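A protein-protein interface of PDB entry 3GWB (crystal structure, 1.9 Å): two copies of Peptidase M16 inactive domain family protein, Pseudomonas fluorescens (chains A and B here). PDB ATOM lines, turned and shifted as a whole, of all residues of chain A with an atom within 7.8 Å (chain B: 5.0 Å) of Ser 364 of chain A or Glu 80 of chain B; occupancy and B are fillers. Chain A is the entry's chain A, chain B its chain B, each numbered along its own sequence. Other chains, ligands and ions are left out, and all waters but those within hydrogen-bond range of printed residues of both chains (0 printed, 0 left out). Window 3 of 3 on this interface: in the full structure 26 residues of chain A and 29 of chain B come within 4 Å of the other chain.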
ATOM      1  N   ALA A  30      10.355  -5.596 -28.350  1.00  0.00           N
ATOM      2  CA  ALA A  30      11.119  -4.465 -27.815  1.00  0.00           C
ATOM      3  C   ALA A  30      11.830  -5.015 -26.590  1.00  0.00           C
ATOM      4  O   ALA A  30      11.211  -5.228 -25.556  1.00  0.00           O
ATOM      5  CB  ALA A  30      10.183  -3.348 -27.421  1.00  0.00           C
ATOM      6  N   GLU A  32      14.476  -3.586 -24.850  1.00  0.00           N
ATOM      7  CA  GLU A  32      15.170  -2.639 -23.972  1.00  0.00           C
ATOM      8  C   GLU A  32      14.867  -2.802 -22.482  1.00  0.00           C
ATOM      9  O   GLU A  32      15.776  -2.776 -21.651  1.00  0.00           O
ATOM     10  CB  GLU A  32      14.873  -1.199 -24.398  1.00  0.00           C
ATOM     11  CG  GLU A  32      13.391  -0.874 -24.610  1.00  0.00           C
ATOM     12  CD  GLU A  32      12.878  -1.248 -26.002  1.00  0.00           C
ATOM     13  OE1 GLU A  32      11.713  -0.908 -26.312  1.00  0.00           O
ATOM     14  OE2 GLU A  32      13.627  -1.872 -26.786  1.00  0.00           O
ATOM     15  N   LEU A  33      13.592  -2.972 -22.147  1.00  0.00           N
ATOM     16  CA  LEU A  33      13.162  -3.128 -20.755  1.00  0.00           C
ATOM     17  C   LEU A  33      12.577  -4.512 -20.502  1.00  0.00           C
ATOM     18  O   LEU A  33      11.914  -5.080 -21.373  1.00  0.00           O
ATOM     19  CB  LEU A  33      12.106  -2.073 -20.416  1.00  0.00           C
ATOM     20  CG  LEU A  33      12.575  -0.628 -20.584  1.00  0.00           C
ATOM     21  CD1 LEU A  33      11.372   0.311 -20.618  1.00  0.00           C
ATOM     22  CD2 LEU A  33      13.529  -0.276 -19.451  1.00  0.00           C
ATOM     23  N   MET A  35       9.997  -5.916 -19.470  1.00  0.00           N
ATOM     24  CA  MET A  35       8.562  -5.843 -19.237  1.00  0.00           C
ATOM     25  C   MET A  35       7.824  -5.790 -20.557  1.00  0.00           C
ATOM     26  O   MET A  35       8.438  -5.703 -21.614  1.00  0.00           O
ATOM     27  CB  MET A  35       8.225  -4.608 -18.394  1.00  0.00           C
ATOM     28  CG  MET A  35       8.954  -3.333 -18.795  1.00  0.00           C
ATOM     29  SD  MET A  35       8.743  -1.968 -17.585  1.00  0.00           S
ATOM     30  CE  MET A  35       8.631  -2.902 -16.033  1.00  0.00           C
ATOM     31  N   ASP A  37       3.656  -4.846 -22.497  1.00  0.00           N
ATOM     32  CA  ASP A  37       2.303  -4.333 -22.404  1.00  0.00           C
ATOM     33  C   ASP A  37       1.385  -5.178 -23.268  1.00  0.00           C
ATOM     34  O   ASP A  37       1.685  -5.432 -24.436  1.00  0.00           O
ATOM     35  CB  ASP A  37       2.240  -2.887 -22.889  1.00  0.00           C
ATOM     36  CG  ASP A  37       2.912  -1.924 -21.934  1.00  0.00           C
ATOM     37  OD1 ASP A  37       2.845  -0.702 -22.174  1.00  0.00           O
ATOM     38  OD2 ASP A  37       3.509  -2.390 -20.944  1.00  0.00           O
ATOM     39  N   VAL A 202       3.366  -5.598 -26.806  1.00  0.00           N
ATOM     40  CA  VAL A 202       4.629  -4.918 -27.037  1.00  0.00           C
ATOM     41  C   VAL A 202       5.575  -5.102 -25.856  1.00  0.00           C
ATOM     42  O   VAL A 202       5.206  -4.833 -24.704  1.00  0.00           O
ATOM     43  CB  VAL A 202       4.441  -3.401 -27.247  1.00  0.00           C
ATOM     44  CG1 VAL A 202       5.782  -2.764 -27.512  1.00  0.00           C
ATOM     45  CG2 VAL A 202       3.483  -3.127 -28.401  1.00  0.00           C
ATOM     46  N   SER A 361      12.257   6.136 -32.779  1.00  0.00           N
ATOM     47  CA  SER A 361      12.691   4.935 -32.069  1.00  0.00           C
ATOM     48  C   SER A 361      12.774   5.207 -30.572  1.00  0.00           C
ATOM     49  O   SER A 361      13.490   4.518 -29.838  1.00  0.00           O
ATOM     50  CB  SER A 361      14.054   4.473 -32.581  1.00  0.00           C
ATOM     51  OG  SER A 361      15.023   5.513 -32.463  1.00  0.00           O
ATOM     52  N   THR A 362      12.027   6.209 -30.128  1.00  0.00           N
ATOM     53  CA  THR A 362      11.988   6.586 -28.722  1.00  0.00           C
ATOM     54  C   THR A 362      10.636   6.230 -28.097  1.00  0.00           C
ATOM     55  O   THR A 362      10.437   6.404 -26.897  1.00  0.00           O
ATOM     56  CB  THR A 362      12.238   8.109 -28.557  1.00  0.00           C
ATOM     57  OG1 THR A 362      11.858   8.521 -27.236  1.00  0.00           O
ATOM     58  CG2 THR A 362      11.429   8.909 -29.588  1.00  0.00           C
ATOM     59  N   ALA A 363       9.716   5.720 -28.911  1.00  0.00           N
ATOM     60  CA  ALA A 363       8.386   5.362 -28.431  1.00  0.00           C
ATOM     61  C   ALA A 363       8.401   4.219 -27.410  1.00  0.00           C
ATOM     62  O   ALA A 363       9.060   3.197 -27.605  1.00  0.00           O
ATOM     63  CB  ALA A 363       7.489   5.008 -29.614  1.00  0.00           C
ATOM     64  N   SER A 364       7.656   4.407 -26.323  1.00  0.00           N
ATOM     65  CA  SER A 364       7.571   3.420 -25.252  1.00  0.00           C
ATOM     66  C   SER A 364       6.621   2.295 -25.623  1.00  0.00           C
ATOM     67  O   SER A 364       5.852   2.410 -26.581  1.00  0.00           O
ATOM     68  CB  SER A 364       7.066   4.082 -23.971  1.00  0.00           C
ATOM     69  OG  SER A 364       5.741   4.568 -24.146  1.00  0.00           O
ATOM     70  N   ASN A 365       6.662   1.215 -24.851  1.00  0.00           N
ATOM     71  CA  ASN A 365       5.781   0.086 -25.104  1.00  0.00           C
ATOM     72  C   ASN A 365       4.311   0.512 -25.013  1.00  0.00           C
ATOM     73  O   ASN A 365       3.496   0.100 -25.834  1.00  0.00           O
ATOM     74  CB  ASN A 365       6.073  -1.060 -24.120  1.00  0.00           C
ATOM     75  CG  ASN A 365       7.463  -1.657 -24.307  1.00  0.00           C
ATOM     76  OD1 ASN A 365       8.135  -1.393 -25.301  1.00  0.00           O
ATOM     77  ND2 ASN A 365       7.891  -2.473 -23.355  1.00  0.00           N
ATOM     78  N   ALA A 366       3.979   1.358 -24.035  1.00  0.00           N
ATOM     79  CA  ALA A 366       2.596   1.814 -23.858  1.00  0.00           C
ATOM     80  C   ALA A 366       2.085   2.621 -25.049  1.00  0.00           C
ATOM     81  O   ALA A 366       0.935   2.466 -25.469  1.00  0.00           O
ATOM     82  CB  ALA A 366       2.471   2.655 -22.583  1.00  0.00           C
ATOM     83  N   ASP A 367       2.934   3.494 -25.584  1.00  0.00           N
ATOM     84  CA  ASP A 367       2.526   4.303 -26.723  1.00  0.00           C
ATOM     85  C   ASP A 367       2.348   3.419 -27.952  1.00  0.00           C
ATOM     86  O   ASP A 367       1.372   3.551 -28.683  1.00  0.00           O
ATOM     87  CB  ASP A 367       3.554   5.396 -27.015  1.00  0.00           C
ATOM     88  CG  ASP A 367       3.495   6.537 -26.010  1.00  0.00           C
ATOM     89  OD1 ASP A 367       2.382   7.059 -25.769  1.00  0.00           O
ATOM     90  OD2 ASP A 367       4.560   6.915 -25.473  1.00  0.00           O
ATOM     91  N   ILE A 368       3.292   2.513 -28.169  1.00  0.00           N
ATOM     92  CA  ILE A 368       3.226   1.610 -29.318  1.00  0.00           C
ATOM     93  C   ILE A 368       2.004   0.700 -29.225  1.00  0.00           C
ATOM     94  O   ILE A 368       1.227   0.595 -30.172  1.00  0.00           O
ATOM     95  CB  ILE A 368       4.503   0.740 -29.424  1.00  0.00           C
ATOM     96  CG1 ILE A 368       5.733   1.638 -29.576  1.00  0.00           C
ATOM     97  CG2 ILE A 368       4.408  -0.202 -30.621  1.00  0.00           C
ATOM     98  CD1 ILE A 368       5.698   2.523 -30.811  1.00  0.00           C
ATOM     99  N   VAL A 369       1.820   0.055 -28.076  1.00  0.00           N
ATOM    100  CA  VAL A 369       0.688  -0.850 -27.903  1.00  0.00           C
ATOM    101  C   VAL A 369      -0.643  -0.124 -28.159  1.00  0.00           C
ATOM    102  O   VAL A 369      -1.594  -0.715 -28.678  1.00  0.00           O
ATOM    103  CB  VAL A 369       0.699  -1.490 -26.486  1.00  0.00           C
ATOM    104  CG1 VAL A 369       0.080  -0.533 -25.451  1.00  0.00           C
ATOM    105  CG2 VAL A 369      -0.039  -2.826 -26.528  1.00  0.00           C
ATOM    106  N   GLY A 370      -0.704   1.158 -27.808  1.00  0.00           N
ATOM    107  CA  GLY A 370      -1.920   1.926 -28.050  1.00  0.00           C
ATOM    108  C   GLY A 370      -2.211   2.053 -29.542  1.00  0.00           C
ATOM    109  O   GLY A 370      -3.351   1.897 -29.985  1.00  0.00           O
ATOM    110  N   ALA B  76      10.556  13.258 -19.316  1.00  0.00           N
ATOM    111  CA  ALA B  76       9.535  12.219 -19.222  1.00  0.00           C
ATOM    112  C   ALA B  76       9.972  10.994 -20.019  1.00  0.00           C
ATOM    113  O   ALA B  76       9.792   9.853 -19.584  1.00  0.00           O
ATOM    114  CB  ALA B  76       8.194  12.747 -19.748  1.00  0.00           C
ATOM    115  N   GLN B  77      10.558  11.242 -21.185  1.00  0.00           N
ATOM    116  CA  GLN B  77      11.026  10.164 -22.044  1.00  0.00           C
ATOM    117  C   GLN B  77      12.192   9.456 -21.357  1.00  0.00           C
ATOM    118  O   GLN B  77      12.341   8.242 -21.466  1.00  0.00           O
ATOM    119  CB  GLN B  77      11.464  10.729 -23.400  1.00  0.00           C
ATOM    120  CG  GLN B  77      11.705   9.671 -24.467  1.00  0.00           C
ATOM    121  CD  GLN B  77      13.167   9.549 -24.868  1.00  0.00           C
ATOM    122  OE1 GLN B  77      14.017   9.135 -24.071  1.00  0.00           O
ATOM    123  NE2 GLN B  77      13.469   9.915 -26.112  1.00  0.00           N
ATOM    124  N   GLY B  78      13.009  10.222 -20.640  1.00  0.00           N
ATOM    125  CA  GLY B  78      14.137   9.637 -19.936  1.00  0.00           C
ATOM    126  C   GLY B  78      13.687   8.597 -18.924  1.00  0.00           C
ATOM    127  O   GLY B  78      14.185   7.470 -18.930  1.00  0.00           O
ATOM    128  N   PHE B  79      12.750   8.966 -18.050  1.00  0.00           N
ATOM    129  CA  PHE B  79      12.244   8.030 -17.045  1.00  0.00           C
ATOM    130  C   PHE B  79      11.536   6.843 -17.700  1.00  0.00           C
ATOM    131  O   PHE B  79      11.791   5.693 -17.353  1.00  0.00           O
ATOM    132  CB  PHE B  79      11.265   8.726 -16.091  1.00  0.00           C
ATOM    133  CG  PHE B  79      11.926   9.676 -15.138  1.00  0.00           C
ATOM    134  CD1 PHE B  79      12.932   9.237 -14.281  1.00  0.00           C
ATOM    135  CD2 PHE B  79      11.536  11.007 -15.088  1.00  0.00           C
ATOM    136  CE1 PHE B  79      13.553  10.122 -13.388  1.00  0.00           C
ATOM    137  CE2 PHE B  79      12.151  11.904 -14.195  1.00  0.00           C
ATOM    138  CZ  PHE B  79      13.157  11.454 -13.343  1.00  0.00           C
ATOM    139  N   GLU B  80      10.643   7.125 -18.642  1.00  0.00           N
ATOM    140  CA  GLU B  80       9.907   6.067 -19.335  1.00  0.00           C
ATOM    141  C   GLU B  80      10.838   5.037 -19.969  1.00  0.00           C
ATOM    142  O   GLU B  80      10.657   3.831 -19.792  1.00  0.00           O
ATOM    143  CB  GLU B  80       8.988   6.670 -20.405  1.00  0.00           C
ATOM    144  CG  GLU B  80       7.658   7.179 -19.850  1.00  0.00           C
ATOM    145  CD  GLU B  80       6.722   7.727 -20.921  1.00  0.00           C
ATOM    146  OE1 GLU B  80       6.538   7.055 -21.962  1.00  0.00           O
ATOM    147  OE2 GLU B  80       6.157   8.823 -20.713  1.00  0.00           O
ATOM    148  N   GLY B  81      11.835   5.518 -20.699  1.00  0.00           N
ATOM    149  CA  GLY B  81      12.777   4.620 -21.349  1.00  0.00           C
ATOM    150  C   GLY B  81      13.564   3.740 -20.395  1.00  0.00           C
ATOM    151  O   GLY B  81      14.059   2.682 -20.786  1.00  0.00           O
ATOM    152  N   LEU B  82      13.681   4.170 -19.141  1.00  0.00           N
ATOM    153  CA  LEU B  82      14.416   3.407 -18.136  1.00  0.00           C
ATOM    154  C   LEU B  82      13.487   2.521 -17.314  1.00  0.00           C
ATOM    155  O   LEU B  82      13.934   1.800 -16.419  1.00  0.00           O
ATOM    156  CB  LEU B  82      15.183   4.359 -17.206  1.00  0.00           C
ATOM    157  CG  LEU B  82      16.320   5.171 -17.834  1.00  0.00           C
ATOM    158  CD1 LEU B  82      16.837   6.206 -16.849  1.00  0.00           C
ATOM    159  CD2 LEU B  82      17.444   4.230 -18.250  1.00  0.00           C
ATOM    160  N   GLY B  83      12.194   2.576 -17.627  1.00  0.00           N
ATOM    161  CA  GLY B  83      11.213   1.778 -16.913  1.00  0.00           C
ATOM    162  C   GLY B  83      10.820   2.394 -15.581  1.00  0.00           C
ATOM    163  O   GLY B  83      10.233   1.723 -14.731  1.00  0.00           O
ATOM    164  N   ALA B  84      11.133   3.675 -15.410  1.00  0.00           N
ATOM    165  CA  ALA B  84      10.839   4.379 -14.168  1.00  0.00           C
ATOM    166  C   ALA B  84       9.606   5.269 -14.249  1.00  0.00           C
ATOM    167  O   ALA B  84       9.205   5.698 -15.329  1.00  0.00           O
ATOM    168  CB  ALA B  84      12.045   5.210 -13.754  1.00  0.00           C
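No position is printed for both chains.
Of the 6 pairs that touch across the chains among the printed residues, none has its exchanged pair printed and touching as well.
Printed residues of chain B within 4 Å of Leu 33 of chain A: Glu 80 (3.7 Å), Gly 81 (3.3 Å), Leu 82 (3.5 Å) and Gly 83 (3.6 Å).
Ser 361 of chain A touches none of the printed residues of chain B.
Ala 363 of chain A touches none of the printed residues of chain B.
Ser 364 of chain A touches one residue of chain B.
Of the printed residues of chain A, Gln 77 of chain B touches Thr 362.
Of chain A, only Leu 33 comes within 4 Å of Gly 81 of chain B.
The nearest printed residue of chain B that does not touch Ser 364 of chain A is Gly 81 of chain B (6.0 Å).
Hydrophobic or aromatic side chains of chain A that line the printed part of chain B: Leu 33.
Among the printed residues, no Asp or Glu carboxylate lies within 4 Å of a Lys or Arg side-chain nitrogen of the other chain.
The side-chain hydroxyl (OG1) of Thr 362 of chain A lies within hydrogen-bond range of the side-chain amide nitrogen (NE2) of Gln 77 of chain B, 2.4 Å away.
The side-chain carboxylate of Glu 80 of chain B sits at hydrogen-bond distance from the side-chain hydroxyl of Ser 364 of chain A, 3.4 Å away.
OD2 of Asp 367 of chain A sits at hydrogen-bond distance from OG of Ser 364 of chain A (2.9 Å).
Among the printed residues, pairs that only touch across the chains: Leu 33 of chain A with Gly 81 of chain B (3.3 Å), Leu 33 of chain A with Leu 82 of chain B (3.5 Å), Leu 33 of chain A with Gly 83 of chain B (3.6 Å) and Leu 33 of chain A with Glu 80 of chain B (3.7 Å).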
